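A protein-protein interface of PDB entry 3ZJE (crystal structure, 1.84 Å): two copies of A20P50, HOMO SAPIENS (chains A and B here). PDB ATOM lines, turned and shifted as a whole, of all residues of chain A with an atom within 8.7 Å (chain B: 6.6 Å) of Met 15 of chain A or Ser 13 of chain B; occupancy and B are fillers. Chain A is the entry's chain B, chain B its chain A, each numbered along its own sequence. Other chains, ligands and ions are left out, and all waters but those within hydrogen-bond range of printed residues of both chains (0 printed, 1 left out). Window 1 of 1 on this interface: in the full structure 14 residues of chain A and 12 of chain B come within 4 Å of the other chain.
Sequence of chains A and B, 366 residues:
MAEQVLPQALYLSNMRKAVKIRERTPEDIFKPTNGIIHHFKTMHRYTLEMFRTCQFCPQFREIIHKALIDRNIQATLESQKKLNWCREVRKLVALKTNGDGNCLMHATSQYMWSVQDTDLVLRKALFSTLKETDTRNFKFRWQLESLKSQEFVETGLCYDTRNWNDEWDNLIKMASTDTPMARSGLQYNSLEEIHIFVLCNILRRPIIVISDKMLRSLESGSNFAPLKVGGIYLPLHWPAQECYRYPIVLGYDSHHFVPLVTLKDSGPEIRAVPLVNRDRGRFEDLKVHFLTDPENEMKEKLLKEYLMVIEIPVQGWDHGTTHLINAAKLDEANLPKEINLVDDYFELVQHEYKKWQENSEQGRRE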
ATOM      1  N   PRO A   7     -17.940   1.980  27.406  1.00  0.00           N
ATOM      2  CA  PRO A   7     -18.663   2.972  26.592  1.00  0.00           C
ATOM      3  C   PRO A   7     -18.447   4.435  27.000  1.00  0.00           C
ATOM      4  O   PRO A   7     -18.232   4.724  28.189  1.00  0.00           O
ATOM      5  CB  PRO A   7     -20.140   2.600  26.800  1.00  0.00           C
ATOM      6  CG  PRO A   7     -20.142   1.223  27.288  1.00  0.00           C
ATOM      7  CD  PRO A   7     -18.816   0.905  27.901  1.00  0.00           C
ATOM      8  N   ALA A   9     -20.598   6.981  26.990  1.00  0.00           N
ATOM      9  CA  ALA A   9     -21.754   7.707  27.518  1.00  0.00           C
ATOM     10  C   ALA A   9     -22.588   6.804  28.387  1.00  0.00           C
ATOM     11  O   ALA A   9     -22.789   5.643  28.035  1.00  0.00           O
ATOM     12  CB  ALA A   9     -22.606   8.297  26.376  1.00  0.00           C
ATOM     13  N   LEU A  10     -23.123   7.334  29.493  1.00  0.00           N
ATOM     14  CA  LEU A  10     -23.805   6.431  30.430  1.00  0.00           C
ATOM     15  C   LEU A  10     -24.880   5.590  29.718  1.00  0.00           C
ATOM     16  O   LEU A  10     -24.976   4.391  29.960  1.00  0.00           O
ATOM     17  CB  LEU A  10     -24.456   7.167  31.579  1.00  0.00           C
ATOM     18  CG  LEU A  10     -23.793   7.246  32.965  1.00  0.00           C
ATOM     19  CD1 LEU A  10     -22.311   6.940  33.010  1.00  0.00           C
ATOM     20  CD2 LEU A  10     -24.088   8.588  33.571  1.00  0.00           C
ATOM     21  N   TYR A  11     -25.669   6.230  28.848  1.00  0.00           N
ATOM     22  CA  TYR A  11     -26.794   5.587  28.147  1.00  0.00           C
ATOM     23  C   TYR A  11     -26.413   4.343  27.337  1.00  0.00           C
ATOM     24  O   TYR A  11     -27.263   3.481  27.063  1.00  0.00           O
ATOM     25  CB  TYR A  11     -27.530   6.605  27.260  1.00  0.00           C
ATOM     26  CG  TYR A  11     -26.991   6.714  25.841  1.00  0.00           C
ATOM     27  CD1 TYR A  11     -25.942   7.571  25.537  1.00  0.00           C
ATOM     28  CD2 TYR A  11     -27.550   5.967  24.801  1.00  0.00           C
ATOM     29  CE1 TYR A  11     -25.453   7.676  24.242  1.00  0.00           C
ATOM     30  CE2 TYR A  11     -27.067   6.062  23.503  1.00  0.00           C
ATOM     31  CZ  TYR A  11     -26.019   6.925  23.229  1.00  0.00           C
ATOM     32  OH  TYR A  11     -25.531   7.013  21.939  1.00  0.00           O
ATOM     33  N   LEU A  12     -25.151   4.248  26.927  1.00  0.00           N
ATOM     34  CA  LEU A  12     -24.753   3.147  26.035  1.00  0.00           C
ATOM     35  C   LEU A  12     -24.495   1.827  26.742  1.00  0.00           C
ATOM     36  O   LEU A  12     -24.282   0.786  26.091  1.00  0.00           O
ATOM     37  CB  LEU A  12     -23.507   3.512  25.258  1.00  0.00           C
ATOM     38  CG  LEU A  12     -23.772   4.749  24.439  1.00  0.00           C
ATOM     39  CD1 LEU A  12     -22.454   5.432  24.292  1.00  0.00           C
ATOM     40  CD2 LEU A  12     -24.207   4.229  23.090  1.00  0.00           C
ATOM     41  N   SER A  13     -24.493   1.872  28.067  1.00  0.00           N
ATOM     42  CA  SER A  13     -24.482   0.649  28.831  1.00  0.00           C
ATOM     43  C   SER A  13     -25.766  -0.112  28.568  1.00  0.00           C
ATOM     44  O   SER A  13     -25.820  -1.301  28.842  1.00  0.00           O
ATOM     45  CB  SER A  13     -24.302   0.904  30.339  1.00  0.00           C
ATOM     46  OG  SER A  13     -25.306   1.765  30.905  1.00  0.00           O
ATOM     47  N   ASN A  14     -26.802   0.579  28.074  1.00  0.00           N
ATOM     48  CA  ASN A  14     -28.106  -0.055  27.898  1.00  0.00           C
ATOM     49  C   ASN A  14     -28.996   0.781  27.009  1.00  0.00           C
ATOM     50  O   ASN A  14     -29.881   1.500  27.526  1.00  0.00           O
ATOM     51  CB  ASN A  14     -28.772  -0.346  29.260  1.00  0.00           C
ATOM     52  CG  ASN A  14     -30.022  -1.215  29.155  1.00  0.00           C
ATOM     53  OD1 ASN A  14     -30.612  -1.363  28.086  1.00  0.00           O
ATOM     54  ND2 ASN A  14     -30.448  -1.771  30.287  1.00  0.00           N
ATOM     55  N   MET A  15     -28.772   0.683  25.689  1.00  0.00           N
ATOM     56  CA  MET A  15     -29.500   1.518  24.727  1.00  0.00           C
ATOM     57  C   MET A  15     -30.994   1.207  24.702  1.00  0.00           C
ATOM     58  O   MET A  15     -31.813   2.100  24.542  1.00  0.00           O
ATOM     59  CB  MET A  15     -28.924   1.424  23.315  1.00  0.00           C
ATOM     60  CG  MET A  15     -27.457   1.793  23.193  1.00  0.00           C
ATOM     61  SD  MET A  15     -26.842   1.513  21.513  1.00  0.00           S
ATOM     62  CE  MET A  15     -27.886   2.647  20.580  1.00  0.00           C
ATOM     63  N   ARG A  16     -31.351  -0.064  24.860  1.00  0.00           N
ATOM     64  CA  ARG A  16     -32.761  -0.417  24.985  1.00  0.00           C
ATOM     65  C   ARG A  16     -33.423   0.361  26.108  1.00  0.00           C
ATOM     66  O   ARG A  16     -34.503   0.903  25.923  1.00  0.00           O
ATOM     67  CB  ARG A  16     -32.971  -1.906  25.237  1.00  0.00           C
ATOM     68  CG  ARG A  16     -34.429  -2.214  25.509  1.00  0.00           C
ATOM     69  CD  ARG A  16     -35.163  -2.001  24.214  1.00  0.00           C
ATOM     70  NE  ARG A  16     -36.589  -2.276  24.266  1.00  0.00           N
ATOM     71  CZ  ARG A  16     -37.501  -1.388  24.656  1.00  0.00           C
ATOM     72  NH1 ARG A  16     -37.111  -0.189  25.094  1.00  0.00           N
ATOM     73  NH2 ARG A  16     -38.794  -1.717  24.646  1.00  0.00           N
ATOM     74  N   LYS A  17     -32.761   0.439  27.263  1.00  0.00           N
ATOM     75  CA  LYS A  17     -33.288   1.188  28.401  1.00  0.00           C
ATOM     76  C   LYS A  17     -33.308   2.699  28.112  1.00  0.00           C
ATOM     77  O   LYS A  17     -34.229   3.404  28.521  1.00  0.00           O
ATOM     78  CB  LYS A  17     -32.502   0.875  29.690  1.00  0.00           C
ATOM     79  CG  LYS A  17     -33.083   1.566  30.952  1.00  0.00           C
ATOM     80  CD  LYS A  17     -32.229   1.321  32.207  1.00  0.00           C
ATOM     81  CE  LYS A  17     -32.521  -0.055  32.776  1.00  0.00           C
ATOM     82  NZ  LYS A  17     -31.585  -0.350  33.912  1.00  0.00           N
ATOM     83  N   ALA A  18     -32.308   3.203  27.401  1.00  0.00           N
ATOM     84  CA  ALA A  18     -32.355   4.605  27.014  1.00  0.00           C
ATOM     85  C   ALA A  18     -33.638   4.916  26.249  1.00  0.00           C
ATOM     86  O   ALA A  18     -34.297   5.942  26.503  1.00  0.00           O
ATOM     87  CB  ALA A  18     -31.102   5.015  26.216  1.00  0.00           C
ATOM     88  N   VAL A  19     -34.016   4.027  25.332  1.00  0.00           N
ATOM     89  CA  VAL A  19     -35.179   4.274  24.511  1.00  0.00           C
ATOM     90  C   VAL A  19     -36.422   4.279  25.374  1.00  0.00           C
ATOM     91  O   VAL A  19     -37.292   5.134  25.200  1.00  0.00           O
ATOM     92  CB  VAL A  19     -35.323   3.257  23.365  1.00  0.00           C
ATOM     93  CG1 VAL A  19     -36.764   3.197  22.880  1.00  0.00           C
ATOM     94  CG2 VAL A  19     -34.388   3.625  22.227  1.00  0.00           C
ATOM     95  N   LYS A  20     -36.474   3.379  26.345  1.00  0.00           N
ATOM     96  CA  LYS A  20     -37.621   3.310  27.219  1.00  0.00           C
ATOM     97  C   LYS A  20     -37.763   4.679  27.954  1.00  0.00           C
ATOM     98  O   LYS A  20     -38.867   5.239  28.025  1.00  0.00           O
ATOM     99  CB  LYS A  20     -37.412   2.212  28.238  1.00  0.00           C
ATOM    100  CG  LYS A  20     -38.525   2.019  29.253  1.00  0.00           C
ATOM    101  CD  LYS A  20     -38.275   0.742  30.045  1.00  0.00           C
ATOM    102  N   ILE A  21     -36.637   5.170  28.458  1.00  0.00           N
ATOM    103  CA  ILE A  21     -36.648   6.434  29.231  1.00  0.00           C
ATOM    104  C   ILE A  21     -37.139   7.557  28.323  1.00  0.00           C
ATOM    105  O   ILE A  21     -38.071   8.313  28.660  1.00  0.00           O
ATOM    106  CB  ILE A  21     -35.246   6.788  29.754  1.00  0.00           C
ATOM    107  CG1 ILE A  21     -34.776   5.776  30.795  1.00  0.00           C
ATOM    108  CG2 ILE A  21     -35.279   8.186  30.412  1.00  0.00           C
ATOM    109  CD1 ILE A  21     -33.330   5.923  31.194  1.00  0.00           C
ATOM    110  N   ARG A  22     -36.510   7.686  27.166  1.00  0.00           N
ATOM    111  CA  ARG A  22     -36.941   8.740  26.262  1.00  0.00           C
ATOM    112  C   ARG A  22     -38.430   8.591  25.925  1.00  0.00           C
ATOM    113  O   ARG A  22     -39.167   9.589  26.007  1.00  0.00           O
ATOM    114  CB  ARG A  22     -36.054   8.831  25.023  1.00  0.00           C
ATOM    115  CG  ARG A  22     -34.714   9.527  25.337  1.00  0.00           C
ATOM    116  CD  ARG A  22     -33.899   9.833  24.094  1.00  0.00           C
ATOM    117  NE  ARG A  22     -32.981   8.743  23.772  1.00  0.00           N
ATOM    118  CZ  ARG A  22     -33.192   7.834  22.821  1.00  0.00           C
ATOM    119  NH1 ARG A  22     -34.300   7.868  22.073  1.00  0.00           N
ATOM    120  NH2 ARG A  22     -32.291   6.882  22.614  1.00  0.00           N
ATOM    121  N   VAL A 115     -30.077  10.485  29.940  1.00  0.00           N
ATOM    122  CA  VAL A 115     -30.126  10.363  28.467  1.00  0.00           C
ATOM    123  C   VAL A 115     -30.039  11.752  27.860  1.00  0.00           C
ATOM    124  O   VAL A 115     -30.409  12.749  28.515  1.00  0.00           O
ATOM    125  CB  VAL A 115     -31.426   9.693  27.918  1.00  0.00           C
ATOM    126  CG1 VAL A 115     -31.529   8.204  28.308  1.00  0.00           C
ATOM    127  CG2 VAL A 115     -32.670  10.460  28.342  1.00  0.00           C
ATOM    128  N   LEU A 341     -29.893   4.197  34.935  1.00  0.00           N
ATOM    129  CA  LEU A 341     -28.935   3.798  33.919  1.00  0.00           C
ATOM    130  C   LEU A 341     -27.482   3.811  34.397  1.00  0.00           C
ATOM    131  O   LEU A 341     -26.591   3.141  33.858  1.00  0.00           O
ATOM    132  CB  LEU A 341     -29.063   4.888  32.888  1.00  0.00           C
ATOM    133  CG  LEU A 341     -28.920   4.452  31.466  1.00  0.00           C
ATOM    134  CD1 LEU A 341     -29.920   5.163  30.542  1.00  0.00           C
ATOM    135  CD2 LEU A 341     -27.574   4.980  31.328  1.00  0.00           C
ATOM    136  N   ASP A 344     -26.487   0.664  35.517  1.00  0.00           N
ATOM    137  CA  ASP A 344     -26.101  -0.323  34.466  1.00  0.00           C
ATOM    138  C   ASP A 344     -24.655  -0.095  34.020  1.00  0.00           C
ATOM    139  O   ASP A 344     -23.861  -1.023  33.984  1.00  0.00           O
ATOM    140  CB  ASP A 344     -27.022  -0.312  33.228  1.00  0.00           C
ATOM    141  CG  ASP A 344     -28.424  -0.792  33.526  1.00  0.00           C
ATOM    142  OD1 ASP A 344     -28.633  -1.481  34.545  1.00  0.00           O
ATOM    143  OD2 ASP A 344     -29.332  -0.492  32.735  1.00  0.00           O
ATOM    144  N   LEU A 348     -21.270  -2.622  34.398  1.00  0.00           N
ATOM    145  CA  LEU A 348     -20.323  -2.930  33.329  1.00  0.00           C
ATOM    146  C   LEU A 348     -18.925  -2.721  33.847  1.00  0.00           C
ATOM    147  O   LEU A 348     -18.070  -3.585  33.724  1.00  0.00           O
ATOM    148  CB  LEU A 348     -20.526  -2.089  32.073  1.00  0.00           C
ATOM    149  CG  LEU A 348     -21.670  -2.382  31.109  1.00  0.00           C
ATOM    150  CD1 LEU A 348     -21.539  -1.502  29.905  1.00  0.00           C
ATOM    151  CD2 LEU A 348     -21.675  -3.847  30.644  1.00  0.00           C
ATOM    152  N   VAL B   5     -27.033   5.118  12.816  1.00  0.00           N
ATOM    153  CA  VAL B   5     -28.482   5.000  13.005  1.00  0.00           C
ATOM    154  C   VAL B   5     -28.812   4.030  14.152  1.00  0.00           C
ATOM    155  O   VAL B   5     -28.703   4.373  15.330  1.00  0.00           O
ATOM    156  CB  VAL B   5     -29.197   4.534  11.699  1.00  0.00           C
ATOM    157  N   LEU B   6     -29.225   2.822  13.790  1.00  0.00           N
ATOM    158  CA  LEU B   6     -29.371   1.709  14.727  1.00  0.00           C
ATOM    159  C   LEU B   6     -28.000   1.427  15.360  1.00  0.00           C
ATOM    160  O   LEU B   6     -27.019   2.082  14.992  1.00  0.00           O
ATOM    161  CB  LEU B   6     -29.891   0.479  13.973  1.00  0.00           C
ATOM    162  N   PRO B   7     -27.904   0.463  16.313  1.00  0.00           N
ATOM    163  CA  PRO B   7     -26.539   0.221  16.783  1.00  0.00           C
ATOM    164  C   PRO B   7     -25.720  -0.256  15.607  1.00  0.00           C
ATOM    165  O   PRO B   7     -26.292  -0.720  14.620  1.00  0.00           O
ATOM    166  CB  PRO B   7     -26.707  -0.892  17.813  1.00  0.00           C
ATOM    167  CG  PRO B   7     -28.092  -0.779  18.275  1.00  0.00           C
ATOM    168  CD  PRO B   7     -28.885  -0.323  17.086  1.00  0.00           C
ATOM    169  N   GLN B   8     -24.407  -0.093  15.680  1.00  0.00           N
ATOM    170  CA  GLN B   8     -23.563  -0.405  14.534  1.00  0.00           C
ATOM    171  C   GLN B   8     -23.285  -1.907  14.472  1.00  0.00           C
ATOM    172  O   GLN B   8     -22.765  -2.399  13.472  1.00  0.00           O
ATOM    173  CB  GLN B   8     -22.268   0.420  14.558  1.00  0.00           C
ATOM    174  N   ALA B   9     -23.668  -2.620  15.532  1.00  0.00           N
ATOM    175  CA  ALA B   9     -23.486  -4.068  15.631  1.00  0.00           C
ATOM    176  C   ALA B   9     -24.244  -4.601  16.857  1.00  0.00           C
ATOM    177  O   ALA B   9     -24.427  -3.882  17.842  1.00  0.00           O
ATOM    178  CB  ALA B   9     -22.025  -4.396  15.752  1.00  0.00           C
ATOM    179  N   LEU B  10     -24.631  -5.875  16.826  1.00  0.00           N
ATOM    180  CA  LEU B  10     -25.591  -6.401  17.798  1.00  0.00           C
ATOM    181  C   LEU B  10     -25.318  -6.119  19.253  1.00  0.00           C
ATOM    182  O   LEU B  10     -26.220  -5.683  19.970  1.00  0.00           O
ATOM    183  CB  LEU B  10     -25.741  -7.894  17.603  1.00  0.00           C
ATOM    184  CG  LEU B  10     -26.689  -8.725  18.424  1.00  0.00           C
ATOM    185  CD1 LEU B  10     -28.087  -8.330  18.196  1.00  0.00           C
ATOM    186  CD2 LEU B  10     -26.437 -10.215  17.926  1.00  0.00           C
ATOM    187  N   TYR B  11     -24.082  -6.360  19.702  1.00  0.00           N
ATOM    188  CA  TYR B  11     -23.787  -6.340  21.141  1.00  0.00           C
ATOM    189  C   TYR B  11     -24.059  -4.970  21.791  1.00  0.00           C
ATOM    190  O   TYR B  11     -24.214  -4.834  23.007  1.00  0.00           O
ATOM    191  CB  TYR B  11     -22.356  -6.873  21.436  1.00  0.00           C
ATOM    192  CG  TYR B  11     -21.209  -5.878  21.230  1.00  0.00           C
ATOM    193  CD1 TYR B  11     -20.848  -5.439  19.950  1.00  0.00           C
ATOM    194  CD2 TYR B  11     -20.474  -5.394  22.318  1.00  0.00           C
ATOM    195  CE1 TYR B  11     -19.786  -4.527  19.758  1.00  0.00           C
ATOM    196  CE2 TYR B  11     -19.409  -4.485  22.142  1.00  0.00           C
ATOM    197  CZ  TYR B  11     -19.069  -4.055  20.860  1.00  0.00           C
ATOM    198  OH  TYR B  11     -18.029  -3.145  20.687  1.00  0.00           O
ATOM    199  N   LEU B  12     -24.133  -3.938  20.976  1.00  0.00           N
ATOM    200  CA  LEU B  12     -24.334  -2.629  21.557  1.00  0.00           C
ATOM    201  C   LEU B  12     -25.758  -2.376  22.048  1.00  0.00           C
ATOM    202  O   LEU B  12     -26.028  -1.295  22.573  1.00  0.00           O
ATOM    203  CB  LEU B  12     -23.938  -1.558  20.551  1.00  0.00           C
ATOM    204  CG  LEU B  12     -22.458  -1.224  20.449  1.00  0.00           C
ATOM    205  CD1 LEU B  12     -21.647  -2.113  21.361  1.00  0.00           C
ATOM    206  CD2 LEU B  12     -21.960  -1.306  19.016  1.00  0.00           C
ATOM    207  N   SER B  13     -26.666  -3.337  21.879  1.00  0.00           N
ATOM    208  CA  SER B  13     -28.087  -3.010  22.045  1.00  0.00           C
ATOM    209  C   SER B  13     -28.517  -2.987  23.523  1.00  0.00           C
ATOM    210  O   SER B  13     -29.449  -2.277  23.911  1.00  0.00           O
ATOM    211  CB  SER B  13     -28.974  -3.933  21.179  1.00  0.00           C
ATOM    212  OG  SER B  13     -29.346  -5.120  21.863  1.00  0.00           O
ATOM    213  N   ASN B  14     -27.814  -3.778  24.333  1.00  0.00           N
ATOM    214  CA  ASN B  14     -28.017  -3.863  25.769  1.00  0.00           C
ATOM    215  C   ASN B  14     -26.776  -4.491  26.412  1.00  0.00           C
ATOM    216  O   ASN B  14     -26.764  -5.710  26.686  1.00  0.00           O
ATOM    217  CB  ASN B  14     -29.263  -4.682  26.092  1.00  0.00           C
ATOM    218  CG  ASN B  14     -29.704  -4.537  27.543  1.00  0.00           C
ATOM    219  OD1 ASN B  14     -28.913  -4.187  28.429  1.00  0.00           O
ATOM    220  ND2 ASN B  14     -30.962  -4.861  27.796  1.00  0.00           N
ATOM    221  N   MET B  15     -25.749  -3.664  26.652  1.00  0.00           N
ATOM    222  CA  MET B  15     -24.459  -4.164  27.149  1.00  0.00           C
ATOM    223  C   MET B  15     -24.593  -4.756  28.544  1.00  0.00           C
ATOM    224  O   MET B  15     -23.971  -5.772  28.871  1.00  0.00           O
ATOM    225  CB  MET B  15     -23.366  -3.103  27.079  1.00  0.00           C
ATOM    226  CG  MET B  15     -22.873  -2.813  25.644  1.00  0.00           C
ATOM    227  SD  MET B  15     -21.580  -1.523  25.556  1.00  0.00           S
ATOM    228  CE  MET B  15     -20.115  -2.558  25.810  1.00  0.00           C
ATOM    229  N   ASN B 340     -32.008 -11.858  25.649  1.00  0.00           N
ATOM    230  CA  ASN B 340     -31.960 -11.821  24.173  1.00  0.00           C
ATOM    231  C   ASN B 340     -31.569 -10.458  23.599  1.00  0.00           C
ATOM    232  O   ASN B 340     -32.397  -9.568  23.528  1.00  0.00           O
ATOM    233  CB  ASN B 340     -33.310 -12.278  23.551  1.00  0.00           C
ATOM    234  CG  ASN B 340     -33.166 -12.715  22.076  1.00  0.00           C
ATOM    235  OD1 ASN B 340     -32.321 -12.195  21.335  1.00  0.00           O
ATOM    236  ND2 ASN B 340     -33.984 -13.694  21.657  1.00  0.00           N
ATOM    237  N   LEU B 341     -30.324 -10.313  23.156  1.00  0.00           N
ATOM    238  CA  LEU B 341     -29.908  -9.071  22.533  1.00  0.00           C
ATOM    239  C   LEU B 341     -30.726  -8.820  21.278  1.00  0.00           C
ATOM    240  O   LEU B 341     -31.044  -7.692  20.945  1.00  0.00           O
ATOM    241  CB  LEU B 341     -28.411  -9.116  22.219  1.00  0.00           C
ATOM    242  CG  LEU B 341     -27.525  -8.313  23.194  1.00  0.00           C
ATOM    243  CD1 LEU B 341     -27.979  -8.521  24.659  1.00  0.00           C
ATOM    244  CD2 LEU B 341     -26.011  -8.622  22.981  1.00  0.00           C
ATOM    245  N   VAL B 342     -31.071  -9.881  20.546  1.00  0.00           N
ATOM    246  CA  VAL B 342     -31.830  -9.638  19.324  1.00  0.00           C
ATOM    247  C   VAL B 342     -33.213  -9.008  19.547  1.00  0.00           C
ATOM    248  O   VAL B 342     -33.680  -8.183  18.762  1.00  0.00           O
ATOM    249  CB  VAL B 342     -31.903 -10.950  18.448  1.00  0.00           C
ATOM    250  CG1 VAL B 342     -32.789 -10.722  17.265  1.00  0.00           C
ATOM    251  CG2 VAL B 342     -30.486 -11.373  17.989  1.00  0.00           C
ATOM    252  N   ASP B 343     -33.894  -9.372  20.621  1.00  0.00           N
ATOM    253  CA  ASP B 343     -35.165  -8.738  20.947  1.00  0.00           C
ATOM    254  C   ASP B 343     -35.002  -7.239  21.277  1.00  0.00           C
ATOM    255  O   ASP B 343     -35.806  -6.386  20.873  1.00  0.00           O
ATOM    256  CB  ASP B 343     -35.701  -9.434  22.167  1.00  0.00           C
ATOM    257  CG  ASP B 343     -37.147  -9.755  22.057  1.00  0.00           C
ATOM    258  OD1 ASP B 343     -37.941  -8.818  22.211  1.00  0.00           O
ATOM    259  OD2 ASP B 343     -37.489 -10.948  21.828  1.00  0.00           O
ATOM    260  N   ASP B 344     -33.941  -6.942  22.016  1.00  0.00           N
ATOM    261  CA  ASP B 344     -33.699  -5.570  22.437  1.00  0.00           C
ATOM    262  C   ASP B 344     -33.325  -4.825  21.183  1.00  0.00           C
ATOM    263  O   ASP B 344     -33.759  -3.691  20.960  1.00  0.00           O
ATOM    264  CB  ASP B 344     -32.585  -5.537  23.489  1.00  0.00           C
ATOM    265  CG  ASP B 344     -33.106  -5.879  24.872  1.00  0.00           C
ATOM    266  OD1 ASP B 344     -34.348  -5.851  25.040  1.00  0.00           O
ATOM    267  OD2 ASP B 344     -32.310  -6.171  25.794  1.00  0.00           O
ATOM    268  N   TYR B 345     -32.559  -5.496  20.327  1.00  0.00           N
ATOM    269  CA  TYR B 345     -32.137  -4.875  19.080  1.00  0.00           C
ATOM    270  C   TYR B 345     -33.376  -4.518  18.238  1.00  0.00           C
ATOM    271  O   TYR B 345     -33.542  -3.386  17.813  1.00  0.00           O
ATOM    272  CB  TYR B 345     -31.207  -5.812  18.306  1.00  0.00           C
ATOM    273  CG  TYR B 345     -30.526  -5.105  17.188  1.00  0.00           C
ATOM    274  CD1 TYR B 345     -31.196  -4.857  16.007  1.00  0.00           C
ATOM    275  CD2 TYR B 345     -29.218  -4.664  17.315  1.00  0.00           C
ATOM    276  CE1 TYR B 345     -30.596  -4.211  14.991  1.00  0.00           C
ATOM    277  CE2 TYR B 345     -28.612  -3.959  16.296  1.00  0.00           C
ATOM    278  CZ  TYR B 345     -29.312  -3.731  15.136  1.00  0.00           C
ATOM    279  OH  TYR B 345     -28.738  -3.057  14.092  1.00  0.00           O
ATOM    280  N   PHE B 346     -34.253  -5.493  18.021  1.00  0.00           N
ATOM    281  CA  PHE B 346     -35.489  -5.260  17.272  1.00  0.00           C
ATOM    282  C   PHE B 346     -36.344  -4.113  17.820  1.00  0.00           C
ATOM    283  O   PHE B 346     -36.936  -3.356  17.034  1.00  0.00           O
ATOM    284  CB  PHE B 346     -36.298  -6.561  17.237  1.00  0.00           C
ATOM    285  CG  PHE B 346     -37.519  -6.502  16.375  1.00  0.00           C
ATOM    286  CD1 PHE B 346     -37.411  -6.557  14.992  1.00  0.00           C
ATOM    287  CD2 PHE B 346     -38.789  -6.432  16.945  1.00  0.00           C
ATOM    288  CE1 PHE B 346     -38.550  -6.530  14.188  1.00  0.00           C
ATOM    289  CE2 PHE B 346     -39.943  -6.391  16.143  1.00  0.00           C
ATOM    290  CZ  PHE B 346     -39.817  -6.441  14.767  1.00  0.00           C
ATOM    291  N   LEU B 348     -35.251  -1.508  19.451  1.00  0.00           N
ATOM    292  CA  LEU B 348     -34.521  -0.315  19.026  1.00  0.00           C
ATOM    293  C   LEU B 348     -34.809  -0.012  17.560  1.00  0.00           C
ATOM    294  O   LEU B 348     -35.021   1.151  17.186  1.00  0.00           O
ATOM    295  CB  LEU B 348     -33.021  -0.502  19.209  1.00  0.00           C
ATOM    296  CG  LEU B 348     -32.218   0.219  20.271  1.00  0.00           C
ATOM    297  CD1 LEU B 348     -33.000   0.460  21.554  1.00  0.00           C
ATOM    298  CD2 LEU B 348     -30.999  -0.579  20.547  1.00  0.00           C
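Among the printed residues, pairs that only touch across the chains: Pro 7 of chain A with Met 15 of chain B, Met 15 of chain A with Ser 13 of chain B, Met 15 of chain A with Leu 348 of chain B, Arg 16 of chain A with Asp 344 of chain B, Arg 16 of chain A with Leu 348 of chain B, Val 19 of chain A with Leu 348 of chain B and Leu 348 of chain A with Met 15 of chain B.
The side-chain amide oxygen (OD1) of Asn 14 of chain B lies close to the side-chain amide oxygen (OD1) of Asn 14 of chain A, 3.3 Å away. The backbone carbonyl oxygen (O) of Ser 13 of chain B lies within hydrogen-bond range of the backbone NH (N) of Arg 16 of chain A, 3.1 Å away. O of Leu 12 of chain B lies close to SD of Met 15 of chain A (3.1 Å). The backbone carbonyl oxygen (O) of Ser 13 of chain A lies within hydrogen-bond range of the backbone NH (N) of Met 15 of chain B (3.2 Å). O of Leu 12 of chain A lies close to SD of Met 15 of chain B (3.6 Å).
Of the printed residues of chain B, Pro 7 of chain A touches Met 15 (3.6 Å). Of chain B, only Leu 12 (3.1 Å), Ser 13 (3.5 Å) and Leu 348 (3.6 Å) come within 4 Å of Met 15 of chain A. Printed residues of chain B within 4 Å of Val 19 of chain A: Leu 348. Leu 6 of chain B touches none of the printed residues of chain A. Of the printed residues of chain A, Leu 12 of chain B touches Met 15. Ser 13 of chain B touches two residues of chain A. Asp 343 of chain B touches none of the printed residues of chain A. The nearest residue of chain B that does not touch Met 15 of chain A is Pro 7 of chain B (4.1 Å). The nearest printed residue of chain B that does not touch Pro 7 of chain A is Leu 12 of chain B (7.0 Å).
Of the 19 printed residues of chain B, 6 touch a printed residue of chain A. Hydrophobic or aromatic side chains of chain B that line the printed part of chain A: Met 15 and Leu 348. Of the 19 printed residues of chain A, 8 touch a printed residue of chain B. Hydrophobic or aromatic side chains of chain A that line the printed part of chain B: Pro 7, Met 15, Val 19 and Leu 348. Among the printed residues, 12 pairs touch across the chains. Among the printed residues, no Asp or Glu carboxylate lies within 4 Å of a Lys or Arg side-chain nitrogen of the other chain.
Pro 7 of chain A touches Met 15 of chain B, but with the chains exchanged Met 15 of chain A does not touch Pro 7 of chain B (4.1 Å). Leu 12 of chain A touches Met 15 of chain B, and with the chains exchanged Met 15 of chain A touches Leu 12 of chain B. Asn 14 of chain B touches its own counterpart, Asn 14 of chain A. Positions printed for both chains: 7, 9, 10, 11, 12, 13, 14, 15, 341, 344 and 348.
OD2 of Asp 344 of chain B sits at hydrogen-bond distance from ND2 of Asn 14 of chain B, 2.7 Å away. The side-chain amide oxygen (OD1) of Asn 14 of chain A lies within hydrogen-bond range of the backbone NH (N) of Lys 17 of chain A, 2.9 Å away. The side-chain hydroxyl of Ser 13 of chain A sits at hydrogen-bond distance from the backbone carbonyl oxygen of Leu 10 of chain A, at 2.8 Å. The side-chain hydroxyl of Ser 13 of chain B is in hydrogen-bond range of the backbone carbonyl oxygen of Leu 341 of chain B (3.2 Å).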
